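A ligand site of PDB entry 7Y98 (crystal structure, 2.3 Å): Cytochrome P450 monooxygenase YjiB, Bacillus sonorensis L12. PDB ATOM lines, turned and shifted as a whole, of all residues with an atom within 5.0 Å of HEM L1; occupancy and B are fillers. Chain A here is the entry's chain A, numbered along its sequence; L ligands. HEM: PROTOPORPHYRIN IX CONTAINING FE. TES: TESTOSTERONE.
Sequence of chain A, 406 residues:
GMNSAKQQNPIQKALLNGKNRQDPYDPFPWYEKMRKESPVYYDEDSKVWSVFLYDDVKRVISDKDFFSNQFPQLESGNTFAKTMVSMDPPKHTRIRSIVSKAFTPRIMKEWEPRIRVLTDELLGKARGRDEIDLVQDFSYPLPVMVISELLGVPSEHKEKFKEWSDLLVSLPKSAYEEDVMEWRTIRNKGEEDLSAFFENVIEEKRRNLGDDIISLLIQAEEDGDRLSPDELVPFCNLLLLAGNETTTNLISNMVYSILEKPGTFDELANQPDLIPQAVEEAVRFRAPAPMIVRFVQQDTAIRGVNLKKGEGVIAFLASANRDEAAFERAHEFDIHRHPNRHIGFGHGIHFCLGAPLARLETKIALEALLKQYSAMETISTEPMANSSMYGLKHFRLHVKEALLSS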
ATOM      1  N   ASN A  69       5.905 -17.605  38.796  1.00  0.00           N
ATOM      2  CA  ASN A  69       7.240 -17.188  38.290  1.00  0.00           C
ATOM      3  C   ASN A  69       7.710 -15.962  39.091  1.00  0.00           C
ATOM      4  O   ASN A  69       8.888 -15.614  38.979  1.00  0.00           O
ATOM      5  CB  ASN A  69       7.199 -16.854  36.803  1.00  0.00           C
ATOM      6  CG  ASN A  69       7.302 -18.064  35.906  1.00  0.00           C
ATOM      7  OD1 ASN A  69       6.468 -18.949  35.947  1.00  0.00           O
ATOM      8  ND2 ASN A  69       8.326 -18.093  35.070  1.00  0.00           N
ATOM      9  N   MET A  84       9.885 -10.453  31.769  1.00  0.00           N
ATOM     10  CA  MET A  84       8.591 -11.170  31.803  1.00  0.00           C
ATOM     11  C   MET A  84       8.807 -12.586  32.350  1.00  0.00           C
ATOM     12  O   MET A  84       7.809 -13.258  32.619  1.00  0.00           O
ATOM     13  CB  MET A  84       7.980 -11.262  30.401  1.00  0.00           C
ATOM     14  CG  MET A  84       9.008 -11.376  29.300  1.00  0.00           C
ATOM     15  SD  MET A  84       8.264 -11.662  27.694  1.00  0.00           S
ATOM     16  CE  MET A  84       9.653 -12.399  26.835  1.00  0.00           C
ATOM     17  N   VAL A  85      10.059 -12.991  32.522  1.00  0.00           N
ATOM     18  CA  VAL A  85      10.388 -14.331  33.088  1.00  0.00           C
ATOM     19  C   VAL A  85       9.918 -14.378  34.539  1.00  0.00           C
ATOM     20  O   VAL A  85       9.444 -15.427  34.972  1.00  0.00           O
ATOM     21  CB  VAL A  85      11.904 -14.623  32.990  1.00  0.00           C
ATOM     22  CG1 VAL A  85      12.257 -15.967  33.605  1.00  0.00           C
ATOM     23  CG2 VAL A  85      12.390 -14.566  31.554  1.00  0.00           C
ATOM     24  N   HIS A  92       2.066 -10.506  32.757  1.00  0.00           N
ATOM     25  CA  HIS A  92       2.861 -11.316  31.795  1.00  0.00           C
ATOM     26  C   HIS A  92       2.128 -11.441  30.463  1.00  0.00           C
ATOM     27  O   HIS A  92       2.729 -11.159  29.435  1.00  0.00           O
ATOM     28  CB  HIS A  92       3.163 -12.692  32.382  1.00  0.00           C
ATOM     29  CG  HIS A  92       3.744 -13.653  31.401  1.00  0.00           C
ATOM     30  ND1 HIS A  92       2.964 -14.423  30.573  1.00  0.00           N
ATOM     31  CD2 HIS A  92       5.023 -13.982  31.112  1.00  0.00           C
ATOM     32  CE1 HIS A  92       3.728 -15.172  29.824  1.00  0.00           C
ATOM     33  NE2 HIS A  92       4.986 -14.922  30.135  1.00  0.00           N
ATOM     34  N   ARG A  96       3.691 -10.520  26.868  1.00  0.00           N
ATOM     35  CA  ARG A  96       3.993 -11.717  26.042  1.00  0.00           C
ATOM     36  C   ARG A  96       3.302 -11.612  24.687  1.00  0.00           C
ATOM     37  O   ARG A  96       3.915 -11.964  23.677  1.00  0.00           O
ATOM     38  CB  ARG A  96       3.563 -12.989  26.775  1.00  0.00           C
ATOM     39  CG  ARG A  96       3.581 -14.230  25.904  1.00  0.00           C
ATOM     40  CD  ARG A  96       4.909 -14.940  25.983  1.00  0.00           C
ATOM     41  NE  ARG A  96       5.079 -15.982  24.984  1.00  0.00           N
ATOM     42  CZ  ARG A  96       5.898 -17.005  25.115  1.00  0.00           C
ATOM     43  NH1 ARG A  96       6.627 -17.127  26.202  1.00  0.00           N
ATOM     44  NH2 ARG A  96       5.994 -17.900  24.155  1.00  0.00           N
ATOM     45  N   PHE A 103       8.408 -12.286  16.589  1.00  0.00           N
ATOM     46  CA  PHE A 103       9.018 -13.637  16.467  1.00  0.00           C
ATOM     47  C   PHE A 103       8.088 -14.614  15.731  1.00  0.00           C
ATOM     48  O   PHE A 103       8.135 -15.807  16.030  1.00  0.00           O
ATOM     49  CB  PHE A 103       9.410 -14.163  17.846  1.00  0.00           C
ATOM     50  CG  PHE A 103      10.491 -13.371  18.535  1.00  0.00           C
ATOM     51  CD1 PHE A 103      10.188 -12.255  19.289  1.00  0.00           C
ATOM     52  CD2 PHE A 103      11.820 -13.742  18.409  1.00  0.00           C
ATOM     53  CE1 PHE A 103      11.189 -11.521  19.913  1.00  0.00           C
ATOM     54  CE2 PHE A 103      12.820 -13.008  19.033  1.00  0.00           C
ATOM     55  CZ  PHE A 103      12.499 -11.904  19.789  1.00  0.00           C
ATOM     56  N   ILE A 147      22.008 -11.935  17.379  1.00  0.00           N
ATOM     57  CA  ILE A 147      21.116 -11.005  18.131  1.00  0.00           C
ATOM     58  C   ILE A 147      21.550  -9.559  17.903  1.00  0.00           C
ATOM     59  O   ILE A 147      20.670  -8.707  17.803  1.00  0.00           O
ATOM     60  CB  ILE A 147      20.970 -11.408  19.610  1.00  0.00           C
ATOM     61  CG1 ILE A 147      19.708 -10.806  20.232  1.00  0.00           C
ATOM     62  CG2 ILE A 147      22.210 -11.072  20.438  1.00  0.00           C
ATOM     63  CD1 ILE A 147      18.439 -11.485  19.781  1.00  0.00           C
ATOM     64  N   PHE A 235      13.371  -5.889  28.034  1.00  0.00           N
ATOM     65  CA  PHE A 235      13.104  -7.012  27.108  1.00  0.00           C
ATOM     66  C   PHE A 235      14.321  -7.218  26.196  1.00  0.00           C
ATOM     67  O   PHE A 235      14.677  -8.374  25.930  1.00  0.00           O
ATOM     68  CB  PHE A 235      11.837  -6.782  26.289  1.00  0.00           C
ATOM     69  CG  PHE A 235      11.598  -7.855  25.269  1.00  0.00           C
ATOM     70  CD1 PHE A 235      11.267  -9.146  25.662  1.00  0.00           C
ATOM     71  CD2 PHE A 235      11.744  -7.603  23.914  1.00  0.00           C
ATOM     72  CE1 PHE A 235      11.073 -10.139  24.724  1.00  0.00           C
ATOM     73  CE2 PHE A 235      11.546  -8.603  22.980  1.00  0.00           C
ATOM     74  CZ  PHE A 235      11.209  -9.867  23.388  1.00  0.00           C
ATOM     75  N   LEU A 238      16.882  -8.992  28.134  1.00  0.00           N
ATOM     76  CA  LEU A 238      16.431 -10.400  28.331  1.00  0.00           C
ATOM     77  C   LEU A 238      16.801 -11.250  27.115  1.00  0.00           C
ATOM     78  O   LEU A 238      17.222 -12.386  27.312  1.00  0.00           O
ATOM     79  CB  LEU A 238      14.927 -10.408  28.600  1.00  0.00           C
ATOM     80  CG  LEU A 238      14.299 -11.792  28.745  1.00  0.00           C
ATOM     81  CD1 LEU A 238      15.023 -12.602  29.805  1.00  0.00           C
ATOM     82  CD2 LEU A 238      12.827 -11.678  29.079  1.00  0.00           C
ATOM     83  N   LEU A 239      16.657 -10.705  25.908  1.00  0.00           N
ATOM     84  CA  LEU A 239      17.023 -11.455  24.666  1.00  0.00           C
ATOM     85  C   LEU A 239      18.494 -11.899  24.774  1.00  0.00           C
ATOM     86  O   LEU A 239      18.767 -13.047  24.435  1.00  0.00           O
ATOM     87  CB  LEU A 239      16.784 -10.570  23.444  1.00  0.00           C
ATOM     88  CG  LEU A 239      15.322 -10.250  23.129  1.00  0.00           C
ATOM     89  CD1 LEU A 239      15.226  -9.342  21.921  1.00  0.00           C
ATOM     90  CD2 LEU A 239      14.533 -11.526  22.885  1.00  0.00           C
ATOM     91  N   ALA A 242      18.734 -14.437  27.905  1.00  0.00           N
ATOM     92  CA  ALA A 242      18.083 -15.755  27.723  1.00  0.00           C
ATOM     93  C   ALA A 242      18.452 -16.442  26.403  1.00  0.00           C
ATOM     94  O   ALA A 242      18.156 -17.635  26.286  1.00  0.00           O
ATOM     95  CB  ALA A 242      16.594 -15.591  27.827  1.00  0.00           C
ATOM     96  N   GLY A 243      19.092 -15.753  25.461  1.00  0.00           N
ATOM     97  CA  GLY A 243      19.370 -16.396  24.167  1.00  0.00           C
ATOM     98  C   GLY A 243      20.843 -16.600  23.849  1.00  0.00           C
ATOM     99  O   GLY A 243      21.121 -17.494  23.039  1.00  0.00           O
ATOM    100  N   THR A 246      22.351 -19.985  26.007  1.00  0.00           N
ATOM    101  CA  THR A 246      21.497 -21.159  25.730  1.00  0.00           C
ATOM    102  C   THR A 246      21.793 -21.662  24.320  1.00  0.00           C
ATOM    103  O   THR A 246      22.045 -22.850  24.148  1.00  0.00           O
ATOM    104  CB  THR A 246      20.012 -20.852  25.922  1.00  0.00           C
ATOM    105  OG1 THR A 246      19.742 -19.665  25.192  1.00  0.00           O
ATOM    106  CG2 THR A 246      19.641 -20.667  27.380  1.00  0.00           C
ATOM    107  N   THR A 247      21.753 -20.764  23.340  1.00  0.00           N
ATOM    108  CA  THR A 247      22.004 -21.129  21.916  1.00  0.00           C
ATOM    109  C   THR A 247      23.431 -21.663  21.782  1.00  0.00           C
ATOM    110  O   THR A 247      23.614 -22.704  21.143  1.00  0.00           O
ATOM    111  CB  THR A 247      21.723 -19.943  20.996  1.00  0.00           C
ATOM    112  OG1 THR A 247      20.444 -19.441  21.372  1.00  0.00           O
ATOM    113  CG2 THR A 247      21.718 -20.327  19.535  1.00  0.00           C
ATOM    114  N   LEU A 250      23.507 -25.056  23.282  1.00  0.00           N
ATOM    115  CA  LEU A 250      22.706 -25.981  22.445  1.00  0.00           C
ATOM    116  C   LEU A 250      23.549 -26.460  21.253  1.00  0.00           C
ATOM    117  O   LEU A 250      23.600 -27.665  21.027  1.00  0.00           O
ATOM    118  CB  LEU A 250      21.437 -25.281  21.965  1.00  0.00           C
ATOM    119  CG  LEU A 250      20.569 -26.107  21.018  1.00  0.00           C
ATOM    120  CD1 LEU A 250      20.328 -27.491  21.589  1.00  0.00           C
ATOM    121  CD2 LEU A 250      19.258 -25.406  20.728  1.00  0.00           C
ATOM    122  N   VAL A 283      18.054 -30.888  22.199  1.00  0.00           N
ATOM    123  CA  VAL A 283      17.441 -30.155  23.346  1.00  0.00           C
ATOM    124  C   VAL A 283      16.945 -31.181  24.374  1.00  0.00           C
ATOM    125  O   VAL A 283      17.028 -30.890  25.559  1.00  0.00           O
ATOM    126  CB  VAL A 283      16.308 -29.210  22.897  1.00  0.00           C
ATOM    127  CG1 VAL A 283      15.445 -28.768  24.069  1.00  0.00           C
ATOM    128  CG2 VAL A 283      16.846 -27.994  22.162  1.00  0.00           C
ATOM    129  N   PRO A 288      20.491 -27.263  27.179  1.00  0.00           N
ATOM    130  CA  PRO A 288      21.379 -26.233  27.684  1.00  0.00           C
ATOM    131  C   PRO A 288      20.852 -25.634  29.001  1.00  0.00           C
ATOM    132  O   PRO A 288      21.668 -25.164  29.739  1.00  0.00           O
ATOM    133  CB  PRO A 288      21.415 -25.178  26.573  1.00  0.00           C
ATOM    134  CG  PRO A 288      20.186 -25.465  25.747  1.00  0.00           C
ATOM    135  CD  PRO A 288      19.959 -26.953  25.862  1.00  0.00           C
ATOM    136  N   ALA A 289      19.539 -25.544  29.190  1.00  0.00           N
ATOM    137  CA  ALA A 289      18.982 -25.019  30.457  1.00  0.00           C
ATOM    138  C   ALA A 289      18.437 -26.198  31.273  1.00  0.00           C
ATOM    139  O   ALA A 289      17.265 -26.547  31.097  1.00  0.00           O
ATOM    140  CB  ALA A 289      17.905 -24.004  30.184  1.00  0.00           C
ATOM    141  N   ILE A 292      14.476 -25.075  35.720  1.00  0.00           N
ATOM    142  CA  ILE A 292      13.636 -23.836  35.697  1.00  0.00           C
ATOM    143  C   ILE A 292      13.174 -23.606  37.134  1.00  0.00           C
ATOM    144  O   ILE A 292      13.045 -24.593  37.875  1.00  0.00           O
ATOM    145  CB  ILE A 292      12.457 -24.010  34.724  1.00  0.00           C
ATOM    146  CG1 ILE A 292      12.377 -22.864  33.715  1.00  0.00           C
ATOM    147  CG2 ILE A 292      11.151 -24.161  35.470  1.00  0.00           C
ATOM    148  CD1 ILE A 292      13.524 -22.848  32.735  1.00  0.00           C
ATOM    149  N   VAL A 293      12.921 -22.353  37.516  1.00  0.00           N
ATOM    150  CA  VAL A 293      12.535 -22.071  38.928  1.00  0.00           C
ATOM    151  C   VAL A 293      11.090 -21.583  39.007  1.00  0.00           C
ATOM    152  O   VAL A 293      10.666 -20.814  38.133  1.00  0.00           O
ATOM    153  CB  VAL A 293      13.526 -21.094  39.578  1.00  0.00           C
ATOM    154  CG1 VAL A 293      13.186 -20.810  41.031  1.00  0.00           C
ATOM    155  CG2 VAL A 293      14.954 -21.579  39.457  1.00  0.00           C
ATOM    156  N   ARG A 294      10.368 -22.057  40.020  1.00  0.00           N
ATOM    157  CA  ARG A 294       8.965 -21.667  40.300  1.00  0.00           C
ATOM    158  C   ARG A 294       8.828 -21.491  41.812  1.00  0.00           C
ATOM    159  O   ARG A 294       9.660 -22.008  42.559  1.00  0.00           O
ATOM    160  CB  ARG A 294       8.002 -22.749  39.819  1.00  0.00           C
ATOM    161  CG  ARG A 294       7.891 -22.863  38.300  1.00  0.00           C
ATOM    162  CD  ARG A 294       7.092 -21.738  37.694  1.00  0.00           C
ATOM    163  NE  ARG A 294       6.889 -21.950  36.267  1.00  0.00           N
ATOM    164  CZ  ARG A 294       7.799 -21.710  35.337  1.00  0.00           C
ATOM    165  NH1 ARG A 294       8.984 -21.253  35.673  1.00  0.00           N
ATOM    166  NH2 ARG A 294       7.509 -21.931  34.070  1.00  0.00           N
ATOM    167  N   LEU A 317      14.418 -29.751  34.073  1.00  0.00           N
ATOM    168  CA  LEU A 317      14.036 -30.069  32.679  1.00  0.00           C
ATOM    169  C   LEU A 317      14.970 -31.167  32.152  1.00  0.00           C
ATOM    170  O   LEU A 317      14.482 -32.082  31.487  1.00  0.00           O
ATOM    171  CB  LEU A 317      14.147 -28.815  31.826  1.00  0.00           C
ATOM    172  CG  LEU A 317      13.379 -27.593  32.309  1.00  0.00           C
ATOM    173  CD1 LEU A 317      13.732 -26.374  31.477  1.00  0.00           C
ATOM    174  CD2 LEU A 317      11.884 -27.841  32.288  1.00  0.00           C
ATOM    175  N   GLY A 344      12.352 -29.200  26.997  1.00  0.00           N
ATOM    176  CA  GLY A 344      13.576 -28.436  27.121  1.00  0.00           C
ATOM    177  C   GLY A 344      13.404 -26.954  26.872  1.00  0.00           C
ATOM    178  O   GLY A 344      14.238 -26.156  27.334  1.00  0.00           O
ATOM    179  N   PHE A 345      12.360 -26.551  26.147  1.00  0.00           N
ATOM    180  CA  PHE A 345      12.015 -25.144  25.995  1.00  0.00           C
ATOM    181  C   PHE A 345      10.971 -24.703  27.017  1.00  0.00           C
ATOM    182  O   PHE A 345      10.439 -23.597  26.909  1.00  0.00           O
ATOM    183  CB  PHE A 345      11.469 -24.875  24.588  1.00  0.00           C
ATOM    184  CG  PHE A 345      12.526 -24.859  23.510  1.00  0.00           C
ATOM    185  CD1 PHE A 345      13.528 -23.895  23.518  1.00  0.00           C
ATOM    186  CD2 PHE A 345      12.489 -25.775  22.479  1.00  0.00           C
ATOM    187  CE1 PHE A 345      14.476 -23.870  22.506  1.00  0.00           C
ATOM    188  CE2 PHE A 345      13.452 -25.754  21.480  1.00  0.00           C
ATOM    189  CZ  PHE A 345      14.445 -24.791  21.497  1.00  0.00           C
ATOM    190  N   GLY A 346      10.691 -25.541  28.012  1.00  0.00           N
ATOM    191  CA  GLY A 346       9.609 -25.275  28.943  1.00  0.00           C
ATOM    192  C   GLY A 346       8.286 -25.851  28.478  1.00  0.00           C
ATOM    193  O   GLY A 346       8.210 -26.692  27.578  1.00  0.00           O
ATOM    194  N   ILE A 349       2.530 -21.029  29.449  1.00  0.00           N
ATOM    195  CA  ILE A 349       2.508 -19.628  29.015  1.00  0.00           C
ATOM    196  C   ILE A 349       3.909 -19.038  28.926  1.00  0.00           C
ATOM    197  O   ILE A 349       4.106 -18.044  28.218  1.00  0.00           O
ATOM    198  CB  ILE A 349       1.632 -18.783  29.956  1.00  0.00           C
ATOM    199  CG1 ILE A 349       2.197 -18.796  31.376  1.00  0.00           C
ATOM    200  CG2 ILE A 349       0.195 -19.269  29.933  1.00  0.00           C
ATOM    201  CD1 ILE A 349       1.569 -17.768  32.291  1.00  0.00           C
ATOM    202  N   HIS A 350       4.873 -19.614  29.626  1.00  0.00           N
ATOM    203  CA  HIS A 350       6.251 -19.146  29.586  1.00  0.00           C
ATOM    204  C   HIS A 350       7.106 -19.913  28.585  1.00  0.00           C
ATOM    205  O   HIS A 350       8.329 -19.775  28.604  1.00  0.00           O
ATOM    206  CB  HIS A 350       6.897 -19.251  30.978  1.00  0.00           C
ATOM    207  CG  HIS A 350       6.513 -18.150  31.915  1.00  0.00           C
ATOM    208  ND1 HIS A 350       7.053 -16.881  31.836  1.00  0.00           N
ATOM    209  CD2 HIS A 350       5.663 -18.130  32.968  1.00  0.00           C
ATOM    210  CE1 HIS A 350       6.544 -16.128  32.791  1.00  0.00           C
ATOM    211  NE2 HIS A 350       5.693 -16.858  33.497  1.00  0.00           N
ATOM    212  N   PHE A 351       6.492 -20.735  27.721  1.00  0.00           N
ATOM    213  CA  PHE A 351       7.234 -21.464  26.707  1.00  0.00           C
ATOM    214  C   PHE A 351       8.182 -20.526  25.987  1.00  0.00           C
ATOM    215  O   PHE A 351       7.784 -19.440  25.560  1.00  0.00           O
ATOM    216  CB  PHE A 351       6.287 -22.124  25.701  1.00  0.00           C
ATOM    217  CG  PHE A 351       6.985 -23.026  24.714  1.00  0.00           C
ATOM    218  CD1 PHE A 351       7.202 -24.357  25.022  1.00  0.00           C
ATOM    219  CD2 PHE A 351       7.430 -22.539  23.495  1.00  0.00           C
ATOM    220  CE1 PHE A 351       7.847 -25.201  24.114  1.00  0.00           C
ATOM    221  CE2 PHE A 351       8.064 -23.374  22.587  1.00  0.00           C
ATOM    222  CZ  PHE A 351       8.277 -24.699  22.901  1.00  0.00           C
ATOM    223  N   CYS A 352       9.446 -20.936  25.877  1.00  0.00           N
ATOM    224  CA  CYS A 352      10.518 -20.050  25.450  1.00  0.00           C
ATOM    225  C   CYS A 352      10.118 -19.247  24.232  1.00  0.00           C
ATOM    226  O   CYS A 352       9.822 -19.815  23.174  1.00  0.00           O
ATOM    227  CB  CYS A 352      11.785 -20.823  25.142  1.00  0.00           C
ATOM    228  SG  CYS A 352      13.077 -19.789  24.399  1.00  0.00           S
ATOM    229  N   LEU A 353      10.110 -17.927  24.382  1.00  0.00           N
ATOM    230  CA  LEU A 353       9.748 -17.041  23.287  1.00  0.00           C
ATOM    231  C   LEU A 353      10.713 -17.166  22.129  1.00  0.00           C
ATOM    232  O   LEU A 353      10.340 -16.941  20.976  1.00  0.00           O
ATOM    233  CB  LEU A 353       9.680 -15.605  23.777  1.00  0.00           C
ATOM    234  CG  LEU A 353       9.309 -14.524  22.771  1.00  0.00           C
ATOM    235  CD1 LEU A 353       7.803 -14.427  22.686  1.00  0.00           C
ATOM    236  CD2 LEU A 353       9.933 -13.210  23.203  1.00  0.00           C
ATOM    237  N   GLY A 354      11.967 -17.511  22.411  1.00  0.00           N
ATOM    238  CA  GLY A 354      13.005 -17.554  21.398  1.00  0.00           C
ATOM    239  C   GLY A 354      13.216 -18.895  20.757  1.00  0.00           C
ATOM    240  O   GLY A 354      14.140 -19.030  19.940  1.00  0.00           O
ATOM    241  N   LEU A 357      13.805 -18.899  17.041  1.00  0.00           N
ATOM    242  CA  LEU A 357      15.113 -18.380  16.677  1.00  0.00           C
ATOM    243  C   LEU A 357      16.215 -19.364  17.040  1.00  0.00           C
ATOM    244  O   LEU A 357      17.148 -19.580  16.265  1.00  0.00           O
ATOM    245  CB  LEU A 357      15.364 -17.031  17.349  1.00  0.00           C
ATOM    246  CG  LEU A 357      16.743 -16.444  17.080  1.00  0.00           C
ATOM    247  CD1 LEU A 357      16.993 -16.345  15.571  1.00  0.00           C
ATOM    248  CD2 LEU A 357      16.883 -15.077  17.730  1.00  0.00           C
ATOM    249  N   ALA A 358      16.129 -19.963  18.230  1.00  0.00           N
ATOM    250  CA  ALA A 358      17.108 -20.979  18.615  1.00  0.00           C
ATOM    251  C   ALA A 358      17.086 -22.143  17.628  1.00  0.00           C
ATOM    252  O   ALA A 358      18.142 -22.633  17.217  1.00  0.00           O
ATOM    253  CB  ALA A 358      16.828 -21.463  20.036  1.00  0.00           C
HETATM  254  CHA HEM L   1      12.108 -18.622  28.239  1.00  0.00           C
HETATM  255  CHB HEM L   1      15.003 -22.372  27.220  1.00  0.00           C
HETATM  256  CHC HEM L   1      17.035 -19.720  23.729  1.00  0.00           C
HETATM  257  CHD HEM L   1      14.302 -15.901  24.895  1.00  0.00           C
HETATM  258  C1A HEM L   1      12.672 -19.872  28.234  1.00  0.00           C
HETATM  259  C2A HEM L   1      12.255 -21.000  29.043  1.00  0.00           C
HETATM  260  C3A HEM L   1      13.058 -22.028  28.754  1.00  0.00           C
HETATM  261  C4A HEM L   1      14.009 -21.594  27.760  1.00  0.00           C
HETATM  262  CMA HEM L   1      13.025 -23.455  29.336  1.00  0.00           C
HETATM  263  CAA HEM L   1      11.073 -21.016  30.048  1.00  0.00           C
HETATM  264  CBA HEM L   1      11.347 -20.142  31.276  1.00  0.00           C
HETATM  265  CGA HEM L   1      10.279 -20.347  32.323  1.00  0.00           C
HETATM  266  O1A HEM L   1       9.303 -21.124  32.095  1.00  0.00           O
HETATM  267  O2A HEM L   1      10.412 -19.758  33.419  1.00  0.00           O
HETATM  268  C1B HEM L   1      15.757 -22.019  26.132  1.00  0.00           C
HETATM  269  C2B HEM L   1      16.596 -22.901  25.346  1.00  0.00           C
HETATM  270  C3B HEM L   1      17.169 -22.171  24.385  1.00  0.00           C
HETATM  271  C4B HEM L   1      16.702 -20.798  24.521  1.00  0.00           C
HETATM  272  CMB HEM L   1      16.808 -24.413  25.572  1.00  0.00           C
HETATM  273  CAB HEM L   1      18.123 -22.763  23.341  1.00  0.00           C
HETATM  274  CBB HEM L   1      18.922 -21.984  22.602  1.00  0.00           C
HETATM  275  C1C HEM L   1      16.442 -18.485  23.717  1.00  0.00           C
HETATM  276  C2C HEM L   1      16.647 -17.456  22.715  1.00  0.00           C
HETATM  277  C3C HEM L   1      15.884 -16.387  23.033  1.00  0.00           C
HETATM  278  C4C HEM L   1      15.182 -16.733  24.251  1.00  0.00           C
HETATM  279  CMC HEM L   1      17.607 -17.644  21.511  1.00  0.00           C
HETATM  280  CAC HEM L   1      15.715 -15.023  22.336  1.00  0.00           C
HETATM  281  CBC HEM L   1      16.287 -14.685  21.172  1.00  0.00           C
HETATM  282  C1D HEM L   1      13.477 -16.311  25.907  1.00  0.00           C
HETATM  283  C2D HEM L   1      12.518 -15.490  26.593  1.00  0.00           C
HETATM  284  C3D HEM L   1      11.911 -16.230  27.513  1.00  0.00           C
HETATM  285  C4D HEM L   1      12.475 -17.570  27.447  1.00  0.00           C
HETATM  286  CMD HEM L   1      12.279 -14.001  26.267  1.00  0.00           C
HETATM  287  CAD HEM L   1      10.811 -15.792  28.505  1.00  0.00           C
HETATM  288  CBD HEM L   1       9.468 -16.381  28.089  1.00  0.00           C
HETATM  289  CGD HEM L   1       8.402 -15.923  29.064  1.00  0.00           C
HETATM  290  O1D HEM L   1       8.745 -15.665  30.249  1.00  0.00           O
HETATM  291  O2D HEM L   1       7.219 -15.831  28.650  1.00  0.00           O
HETATM  292  NA  HEM L   1      13.751 -20.280  27.462  1.00  0.00           N
HETATM  293  NB  HEM L   1      15.849 -20.746  25.603  1.00  0.00           N
HETATM  294  NC  HEM L   1      15.525 -18.007  24.635  1.00  0.00           N
HETATM  295  ND  HEM L   1      13.436 -17.586  26.453  1.00  0.00           N
HETATM  296 FE   HEM L   1      14.591 -19.174  25.968  1.00  0.00          FE
HETATM  297  C1  TES L   2      19.198 -19.345  36.756  1.00  0.00           C
HETATM  298  C2  TES L   2      19.531 -19.405  38.243  1.00  0.00           C
HETATM  299  C3  TES L   2      18.508 -18.691  39.046  1.00  0.00           C
HETATM  300  O3  TES L   2      18.822 -18.064  40.040  1.00  0.00           O
HETATM  301  C4  TES L   2      17.133 -18.766  38.567  1.00  0.00           C
HETATM  302  C5  TES L   2      16.791 -19.069  37.304  1.00  0.00           C
HETATM  303  C6  TES L   2      15.406 -18.774  36.782  1.00  0.00           C
HETATM  304  C7  TES L   2      15.428 -18.208  35.374  1.00  0.00           C
HETATM  305  C8  TES L   2      16.147 -19.153  34.412  1.00  0.00           C
HETATM  306  C9  TES L   2      17.600 -19.358  34.867  1.00  0.00           C
HETATM  307  C10 TES L   2      17.766 -19.762  36.375  1.00  0.00           C
HETATM  308  C11 TES L   2      18.380 -20.281  33.904  1.00  0.00           C
HETATM  309  C12 TES L   2      18.301 -19.880  32.435  1.00  0.00           C
HETATM  310  C13 TES L   2      16.855 -19.619  31.989  1.00  0.00           C
HETATM  311  C14 TES L   2      16.207 -18.630  32.978  1.00  0.00           C
HETATM  312  C15 TES L   2      14.937 -18.150  32.257  1.00  0.00           C
HETATM  313  C16 TES L   2      15.252 -18.349  30.750  1.00  0.00           C
HETATM  314  C17 TES L   2      16.719 -18.809  30.702  1.00  0.00           C
HETATM  315  O17 TES L   2      17.067 -19.501  29.514  1.00  0.00           O
HETATM  316  C18 TES L   2      16.070 -20.926  31.840  1.00  0.00           C
HETATM  317  C19 TES L   2      17.556 -21.288  36.568  1.00  0.00           C
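The side-chain amide nitrogen (ND2) of Asn 69 is in hydrogen-bond range of the backbone carbonyl oxygen (O) of Val 85 (2.9 Å).
The side-chain sulfur of Cys 352 lies close to the backbone NH of Gly 354.
A ring nitrogen (NE2) of His 350 lies close to the side-chain amide nitrogen (ND2) of Asn 69 (3.3 Å).
OD1 of Asn 69 sits at hydrogen-bond distance from NE of Arg 294, at 3.0 Å.
NE2 of His 92 sits close to ND1 of His 350, 3.3 Å away.
The backbone carbonyl oxygen (O) of Phe 345 lies within hydrogen-bond range of the backbone NH (N) of Cys 352.
The side-chain hydroxyl of Thr 247 sits at hydrogen-bond distance from the backbone carbonyl oxygen of Gly 243, at 2.7 Å.
O of Gly 243 lies within hydrogen-bond range of OG1 of Thr 246.
An iron atom (FE) of HEM L1 is bound by the side-chain sulfur (SG) of Cys 352.
A ring nitrogen (ND1) of His 350 lies within hydrogen-bond range of an oxygen (O1D) of HEM L1, at 2.6 Å.
O1A of HEM L1 lies within salt-bridge range of NH2 of Arg 294, 2.8 Å away.
An oxygen (O2D) of HEM L1 lies within salt-bridge range of the guanidinium group (NH1) of Arg 96 (2.8 Å).
The side-chain amide nitrogen of Asn 69 sits at hydrogen-bond distance from an oxygen (O2A) of HEM L1 (3.1 Å).
An oxygen (O2D) of HEM L1 sits at hydrogen-bond distance from a ring nitrogen (NE2) of His 92 (2.8 Å).
The backbone carbonyl oxygen (O) of Ala 242 lies close to a nitrogen (NC) of HEM L1, 3.1 Å away.
Residues that only touch HEM L1: Thr 246, Met 84, Thr 247, Gly 243, Phe 345, Ala 358, Gly 346, Ile 292, Gly 354, Leu 357, Val 85, Pro 288, Gly 344, Leu 238, Leu 317, Leu 239, Ile 349, Leu 250 and Leu 353.
Hydrophobic or aromatic side chains within 4 Å of HEM L1: Met 84, Val 85, His 92, Leu 238, Leu 239, Ala 242, Leu 250, Pro 288, Ile 292, Leu 317, Phe 345, His 350, Leu 353, Leu 357 and Ala 358.
Of the 33 residues printed, 26 come within 4 Å of HEM L1.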
